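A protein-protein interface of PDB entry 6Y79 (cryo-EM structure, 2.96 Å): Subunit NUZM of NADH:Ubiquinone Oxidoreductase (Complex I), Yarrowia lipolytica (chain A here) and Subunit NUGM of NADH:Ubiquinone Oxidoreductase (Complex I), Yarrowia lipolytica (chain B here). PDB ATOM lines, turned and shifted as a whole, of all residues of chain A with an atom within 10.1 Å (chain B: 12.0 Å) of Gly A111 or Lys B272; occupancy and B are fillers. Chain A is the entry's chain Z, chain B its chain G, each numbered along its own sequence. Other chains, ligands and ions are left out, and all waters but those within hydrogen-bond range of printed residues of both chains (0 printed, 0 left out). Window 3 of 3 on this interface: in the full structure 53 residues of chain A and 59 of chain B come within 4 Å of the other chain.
The backbone carbonyl oxygen of Gly A111 is in hydrogen-bond range of the side-chain hydroxyl of Thr A115, at 3.3 Å.
Ser A102 touches Pro B269. CA of Pro B269 touches CG of Glu A103, 3.9 Å away. Pro B271 touches Gly A111 (CB to O, 3.5 Å). Gly A111 touches Lys B272. CG of Pro B271 touches C of Gly A114, at 3.95 Å. Leu A118 touches Pro B271.
Of the 5 printed residues of chain B, 4 touch a printed residue of chain A. Printed residues of chain B that touch a printed residue of chain A: Leu B268, Pro B269, Pro B271 and Lys B272. Hydrophobic or aromatic side chains of chain B that line the printed part of chain A: Pro B269 and Pro B271. Along chain B the printed residues that touch a printed residue of chain A span positions 268 to 272. Hydrophobic or aromatic side chains of chain A that line the printed part of chain B: Leu A118. Among the printed residues, 7 pairs touch across the chains. Among the printed residues, no Asp or Glu carboxylate lies within 4 Å of a Lys or Arg side-chain nitrogen of the other chain.
Of the printed residues of chain B, Gly A111 touches Pro B271 (3.5 Å) and Lys B272 (3.9 Å). Lys B272 touches just one residue of chain A: Gly A111. No residue of chain B comes within 4 Å of Ile A108. No residue of chain B comes within 4 Å of Ala A109. No residue of chain B comes within 4 Å of Asp A110. Ala A113 touches none of the printed residues of chain B. Of chain B, only Pro B271 comes within 4 Å of Gly A114. No residue of chain B comes within 4 Å of Thr A115. Of the printed residues of chain B, Leu A118 touches Pro B271. Of the printed residues of chain B, Glu A103 touches Leu B268 (3.3 Å) and Pro B269 (3.9 Å). Of the printed residues of chain A, Pro B269 touches Ser A102 and Glu A103. Printed residues of chain B within 4 Å of Ser A102: Pro B269. Pro A106 touches none of the printed residues of chain B. Leu A100 touches none of the printed residues of chain B. The nearest residue of chain A that does not touch Lys B272 is Ile A108 (4.8 Å). The nearest printed residue of chain A that does not touch Pro B269 is Leu A100 (4.1 Å).
The side-chain carboxylate (OE2) of Glu A103 sits close to the backbone carbonyl oxygen (O) of Leu B268 (3.3 Å).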
ATOM      1  N   LEU A 100      -8.322  -3.908  19.097  1.00  0.00           N
ATOM      2  CA  LEU A 100      -8.645  -4.334  20.451  1.00  0.00           C
ATOM      3  C   LEU A 100      -7.386  -4.730  21.204  1.00  0.00           C
ATOM      4  O   LEU A 100      -7.183  -4.338  22.355  1.00  0.00           O
ATOM      5  CB  LEU A 100      -9.659  -5.467  20.422  1.00  0.00           C
ATOM      6  CG  LEU A 100     -11.112  -5.050  20.359  1.00  0.00           C
ATOM      7  CD1 LEU A 100     -11.573  -4.636  18.975  1.00  0.00           C
ATOM      8  CD2 LEU A 100     -11.847  -6.262  20.800  1.00  0.00           C
ATOM      9  N   SER A 102      -4.499  -7.942  22.070  1.00  0.00           N
ATOM     10  CA  SER A 102      -3.945  -9.284  22.019  1.00  0.00           C
ATOM     11  C   SER A 102      -4.157  -9.915  23.383  1.00  0.00           C
ATOM     12  O   SER A 102      -4.533  -9.241  24.337  1.00  0.00           O
ATOM     13  CB  SER A 102      -2.455  -9.261  21.665  1.00  0.00           C
ATOM     14  OG  SER A 102      -2.235  -8.748  20.363  1.00  0.00           O
ATOM     15  N   GLU A 103      -3.915 -11.212  23.478  1.00  0.00           N
ATOM     16  CA  GLU A 103      -3.988 -11.810  24.802  1.00  0.00           C
ATOM     17  C   GLU A 103      -2.727 -11.574  25.612  1.00  0.00           C
ATOM     18  O   GLU A 103      -2.782 -11.608  26.844  1.00  0.00           O
ATOM     19  CB  GLU A 103      -4.273 -13.300  24.715  1.00  0.00           C
ATOM     20  CG  GLU A 103      -5.674 -13.588  24.260  1.00  0.00           C
ATOM     21  CD  GLU A 103      -5.969 -15.037  24.242  1.00  0.00           C
ATOM     22  OE1 GLU A 103      -5.062 -15.854  24.559  1.00  0.00           O
ATOM     23  OE2 GLU A 103      -7.132 -15.412  23.933  1.00  0.00           O
ATOM     24  N   PRO A 106      -3.526  -6.835  26.119  1.00  0.00           N
ATOM     25  CA  PRO A 106      -4.928  -6.386  26.074  1.00  0.00           C
ATOM     26  C   PRO A 106      -5.024  -4.879  26.270  1.00  0.00           C
ATOM     27  O   PRO A 106      -4.660  -4.337  27.316  1.00  0.00           O
ATOM     28  CB  PRO A 106      -5.579  -7.161  27.230  1.00  0.00           C
ATOM     29  CG  PRO A 106      -4.481  -7.444  28.172  1.00  0.00           C
ATOM     30  CD  PRO A 106      -3.195  -7.493  27.402  1.00  0.00           C
ATOM     31  N   ARG A 107      -5.538  -4.205  25.249  1.00  0.00           N
ATOM     32  CA  ARG A 107      -5.868  -2.785  25.289  1.00  0.00           C
ATOM     33  C   ARG A 107      -7.357  -2.587  25.491  1.00  0.00           C
ATOM     34  O   ARG A 107      -7.959  -1.663  24.941  1.00  0.00           O
ATOM     35  CB  ARG A 107      -5.409  -2.090  24.012  1.00  0.00           C
ATOM     36  CG  ARG A 107      -3.970  -2.348  23.652  1.00  0.00           C
ATOM     37  CD  ARG A 107      -3.603  -1.687  22.337  1.00  0.00           C
ATOM     38  NE  ARG A 107      -2.205  -1.948  22.027  1.00  0.00           N
ATOM     39  CZ  ARG A 107      -1.785  -2.952  21.267  1.00  0.00           C
ATOM     40  NH1 ARG A 107      -2.658  -3.781  20.719  1.00  0.00           N
ATOM     41  NH2 ARG A 107      -0.491  -3.134  21.069  1.00  0.00           N
ATOM     42  N   ILE A 108      -7.972  -3.467  26.270  1.00  0.00           N
ATOM     43  CA  ILE A 108      -9.411  -3.488  26.470  1.00  0.00           C
ATOM     44  C   ILE A 108      -9.689  -3.374  27.962  1.00  0.00           C
ATOM     45  O   ILE A 108      -9.369  -4.286  28.738  1.00  0.00           O
ATOM     46  CB  ILE A 108     -10.028  -4.763  25.869  1.00  0.00           C
ATOM     47  CG1 ILE A 108      -9.937  -4.731  24.346  1.00  0.00           C
ATOM     48  CG2 ILE A 108     -11.481  -4.935  26.230  1.00  0.00           C
ATOM     49  CD1 ILE A 108     -10.556  -3.483  23.733  1.00  0.00           C
ATOM     50  N   ALA A 109     -10.253  -2.239  28.359  1.00  0.00           N
ATOM     51  CA  ALA A 109     -11.034  -2.122  29.581  1.00  0.00           C
ATOM     52  C   ALA A 109     -12.500  -2.296  29.194  1.00  0.00           C
ATOM     53  O   ALA A 109     -12.811  -2.632  28.044  1.00  0.00           O
ATOM     54  CB  ALA A 109     -10.810  -0.771  30.280  1.00  0.00           C
ATOM     55  N   ASP A 110     -13.391  -2.106  30.177  1.00  0.00           N
ATOM     56  CA  ASP A 110     -14.847  -2.115  30.011  1.00  0.00           C
ATOM     57  C   ASP A 110     -15.325  -3.455  29.448  1.00  0.00           C
ATOM     58  O   ASP A 110     -15.821  -3.501  28.332  1.00  0.00           O
ATOM     59  CB  ASP A 110     -15.316  -1.013  29.063  1.00  0.00           C
ATOM     60  CG  ASP A 110     -15.540   0.310  29.739  1.00  0.00           C
ATOM     61  OD1 ASP A 110     -15.542   0.415  30.993  1.00  0.00           O
ATOM     62  OD2 ASP A 110     -15.730   1.285  28.969  1.00  0.00           O
ATOM     63  N   GLY A 111     -15.119  -4.544  30.219  1.00  0.00           N
ATOM     64  CA  GLY A 111     -15.374  -5.896  29.691  1.00  0.00           C
ATOM     65  C   GLY A 111     -16.786  -6.114  29.182  1.00  0.00           C
ATOM     66  O   GLY A 111     -16.976  -6.637  28.069  1.00  0.00           O
ATOM     67  N   GLU A 112     -17.775  -5.623  29.942  1.00  0.00           N
ATOM     68  CA  GLU A 112     -19.162  -5.541  29.509  1.00  0.00           C
ATOM     69  C   GLU A 112     -19.318  -4.741  28.219  1.00  0.00           C
ATOM     70  O   GLU A 112     -20.076  -5.143  27.332  1.00  0.00           O
ATOM     71  CB  GLU A 112     -19.978  -4.917  30.643  1.00  0.00           C
ATOM     72  CG  GLU A 112     -21.452  -4.790  30.379  1.00  0.00           C
ATOM     73  CD  GLU A 112     -22.157  -6.123  30.306  1.00  0.00           C
ATOM     74  OE1 GLU A 112     -21.718  -7.089  30.967  1.00  0.00           O
ATOM     75  OE2 GLU A 112     -23.146  -6.202  29.555  1.00  0.00           O
ATOM     76  N   ALA A 113     -18.611  -3.622  28.089  1.00  0.00           N
ATOM     77  CA  ALA A 113     -18.669  -2.859  26.849  1.00  0.00           C
ATOM     78  C   ALA A 113     -17.618  -3.308  25.840  1.00  0.00           C
ATOM     79  O   ALA A 113     -17.716  -2.958  24.662  1.00  0.00           O
ATOM     80  CB  ALA A 113     -18.512  -1.367  27.143  1.00  0.00           C
ATOM     81  N   GLY A 114     -16.617  -4.076  26.279  1.00  0.00           N
ATOM     82  CA  GLY A 114     -15.623  -4.605  25.363  1.00  0.00           C
ATOM     83  C   GLY A 114     -16.165  -5.698  24.484  1.00  0.00           C
ATOM     84  O   GLY A 114     -15.669  -5.894  23.372  1.00  0.00           O
ATOM     85  N   THR A 115     -17.193  -6.411  24.953  1.00  0.00           N
ATOM     86  CA  THR A 115     -17.890  -7.337  24.058  1.00  0.00           C
ATOM     87  C   THR A 115     -18.578  -6.605  22.901  1.00  0.00           C
ATOM     88  O   THR A 115     -18.472  -7.017  21.740  1.00  0.00           O
ATOM     89  CB  THR A 115     -18.892  -8.168  24.852  1.00  0.00           C
ATOM     90  OG1 THR A 115     -18.198  -8.860  25.895  1.00  0.00           O
ATOM     91  CG2 THR A 115     -19.568  -9.188  23.953  1.00  0.00           C
ATOM     92  N   LYS A 116     -19.247  -5.488  23.178  1.00  0.00           N
ATOM     93  CA  LYS A 116     -19.878  -4.771  22.075  1.00  0.00           C
ATOM     94  C   LYS A 116     -18.868  -3.937  21.292  1.00  0.00           C
ATOM     95  O   LYS A 116     -19.136  -3.557  20.145  1.00  0.00           O
ATOM     96  CB  LYS A 116     -21.038  -3.931  22.598  1.00  0.00           C
ATOM     97  CG  LYS A 116     -22.100  -4.797  23.255  1.00  0.00           C
ATOM     98  CD  LYS A 116     -23.229  -3.988  23.847  1.00  0.00           C
ATOM     99  CE  LYS A 116     -23.944  -4.781  24.930  1.00  0.00           C
ATOM    100  NZ  LYS A 116     -23.772  -4.168  26.276  1.00  0.00           N
ATOM    101  N   ALA A 117     -17.703  -3.654  21.879  1.00  0.00           N
ATOM    102  CA  ALA A 117     -16.603  -3.083  21.108  1.00  0.00           C
ATOM    103  C   ALA A 117     -15.987  -4.110  20.162  1.00  0.00           C
ATOM    104  O   ALA A 117     -15.527  -3.746  19.075  1.00  0.00           O
ATOM    105  CB  ALA A 117     -15.540  -2.517  22.046  1.00  0.00           C
ATOM    106  N   LEU A 118     -15.939  -5.381  20.576  1.00  0.00           N
ATOM    107  CA  LEU A 118     -15.630  -6.488  19.675  1.00  0.00           C
ATOM    108  C   LEU A 118     -16.644  -6.588  18.549  1.00  0.00           C
ATOM    109  O   LEU A 118     -16.279  -6.883  17.398  1.00  0.00           O
ATOM    110  CB  LEU A 118     -15.665  -7.814  20.437  1.00  0.00           C
ATOM    111  CG  LEU A 118     -14.591  -8.539  21.225  1.00  0.00           C
ATOM    112  CD1 LEU A 118     -15.255  -9.363  22.324  1.00  0.00           C
ATOM    113  CD2 LEU A 118     -13.799  -9.429  20.288  1.00  0.00           C
ATOM    114  N   ALA A 119     -17.918  -6.371  18.891  1.00  0.00           N
ATOM    115  CA  ALA A 119     -19.030  -6.766  18.036  1.00  0.00           C
ATOM    116  C   ALA A 119     -19.046  -6.034  16.701  1.00  0.00           C
ATOM    117  O   ALA A 119     -19.234  -6.681  15.677  1.00  0.00           O
ATOM    118  CB  ALA A 119     -20.358  -6.552  18.771  1.00  0.00           C
ATOM    119  N   LEU B 268      -7.457 -12.803  19.720  1.00  0.00           N
ATOM    120  CA  LEU B 268      -8.192 -11.664  20.243  1.00  0.00           C
ATOM    121  C   LEU B 268      -8.266 -11.721  21.765  1.00  0.00           C
ATOM    122  O   LEU B 268      -8.432 -12.802  22.337  1.00  0.00           O
ATOM    123  CB  LEU B 268      -9.600 -11.641  19.653  1.00  0.00           C
ATOM    124  CG  LEU B 268      -9.637 -11.397  18.148  1.00  0.00           C
ATOM    125  CD1 LEU B 268     -11.036 -11.571  17.594  1.00  0.00           C
ATOM    126  CD2 LEU B 268      -9.128 -10.016  17.870  1.00  0.00           C
ATOM    127  N   PRO B 269      -8.122 -10.584  22.444  1.00  0.00           N
ATOM    128  CA  PRO B 269      -8.172 -10.593  23.907  1.00  0.00           C
ATOM    129  C   PRO B 269      -9.581 -10.844  24.395  1.00  0.00           C
ATOM    130  O   PRO B 269     -10.550 -10.320  23.842  1.00  0.00           O
ATOM    131  CB  PRO B 269      -7.709  -9.187  24.286  1.00  0.00           C
ATOM    132  CG  PRO B 269      -8.054  -8.351  23.116  1.00  0.00           C
ATOM    133  CD  PRO B 269      -7.934  -9.225  21.905  1.00  0.00           C
ATOM    134  N   THR B 270      -9.702 -11.666  25.422  1.00  0.00           N
ATOM    135  CA  THR B 270     -10.991 -11.730  26.073  1.00  0.00           C
ATOM    136  C   THR B 270     -11.152 -10.484  26.941  1.00  0.00           C
ATOM    137  O   THR B 270     -10.170  -9.982  27.506  1.00  0.00           O
ATOM    138  CB  THR B 270     -11.175 -13.039  26.867  1.00  0.00           C
ATOM    139  OG1 THR B 270     -12.571 -13.250  27.115  1.00  0.00           O
ATOM    140  CG2 THR B 270     -10.408 -13.074  28.186  1.00  0.00           C
ATOM    141  N   PRO B 271     -12.330  -9.875  26.941  1.00  0.00           N
ATOM    142  CA  PRO B 271     -12.525  -8.664  27.735  1.00  0.00           C
ATOM    143  C   PRO B 271     -12.515  -8.983  29.220  1.00  0.00           C
ATOM    144  O   PRO B 271     -12.834 -10.101  29.634  1.00  0.00           O
ATOM    145  CB  PRO B 271     -13.891  -8.154  27.267  1.00  0.00           C
ATOM    146  CG  PRO B 271     -14.031  -8.713  25.894  1.00  0.00           C
ATOM    147  CD  PRO B 271     -13.425 -10.074  25.979  1.00  0.00           C
ATOM    148  N   LYS B 272     -12.132  -7.975  30.008  1.00  0.00           N
ATOM    149  CA  LYS B 272     -11.744  -8.102  31.419  1.00  0.00           C
ATOM    150  C   LYS B 272     -10.668  -9.167  31.611  1.00  0.00           C
ATOM    151  O   LYS B 272      -9.621  -8.903  32.202  1.00  0.00           O
ATOM    152  CB  LYS B 272     -12.947  -8.411  32.319  1.00  0.00           C
ATOM    153  CG  LYS B 272     -12.568  -8.657  33.770  1.00  0.00           C
ATOM    154  CD  LYS B 272     -13.569  -9.554  34.476  1.00  0.00           C
ATOM    155  CE  LYS B 272     -14.980  -9.009  34.361  1.00  0.00           C
ATOM    156  NZ  LYS B 272     -15.938  -9.788  35.188  1.00  0.00           N
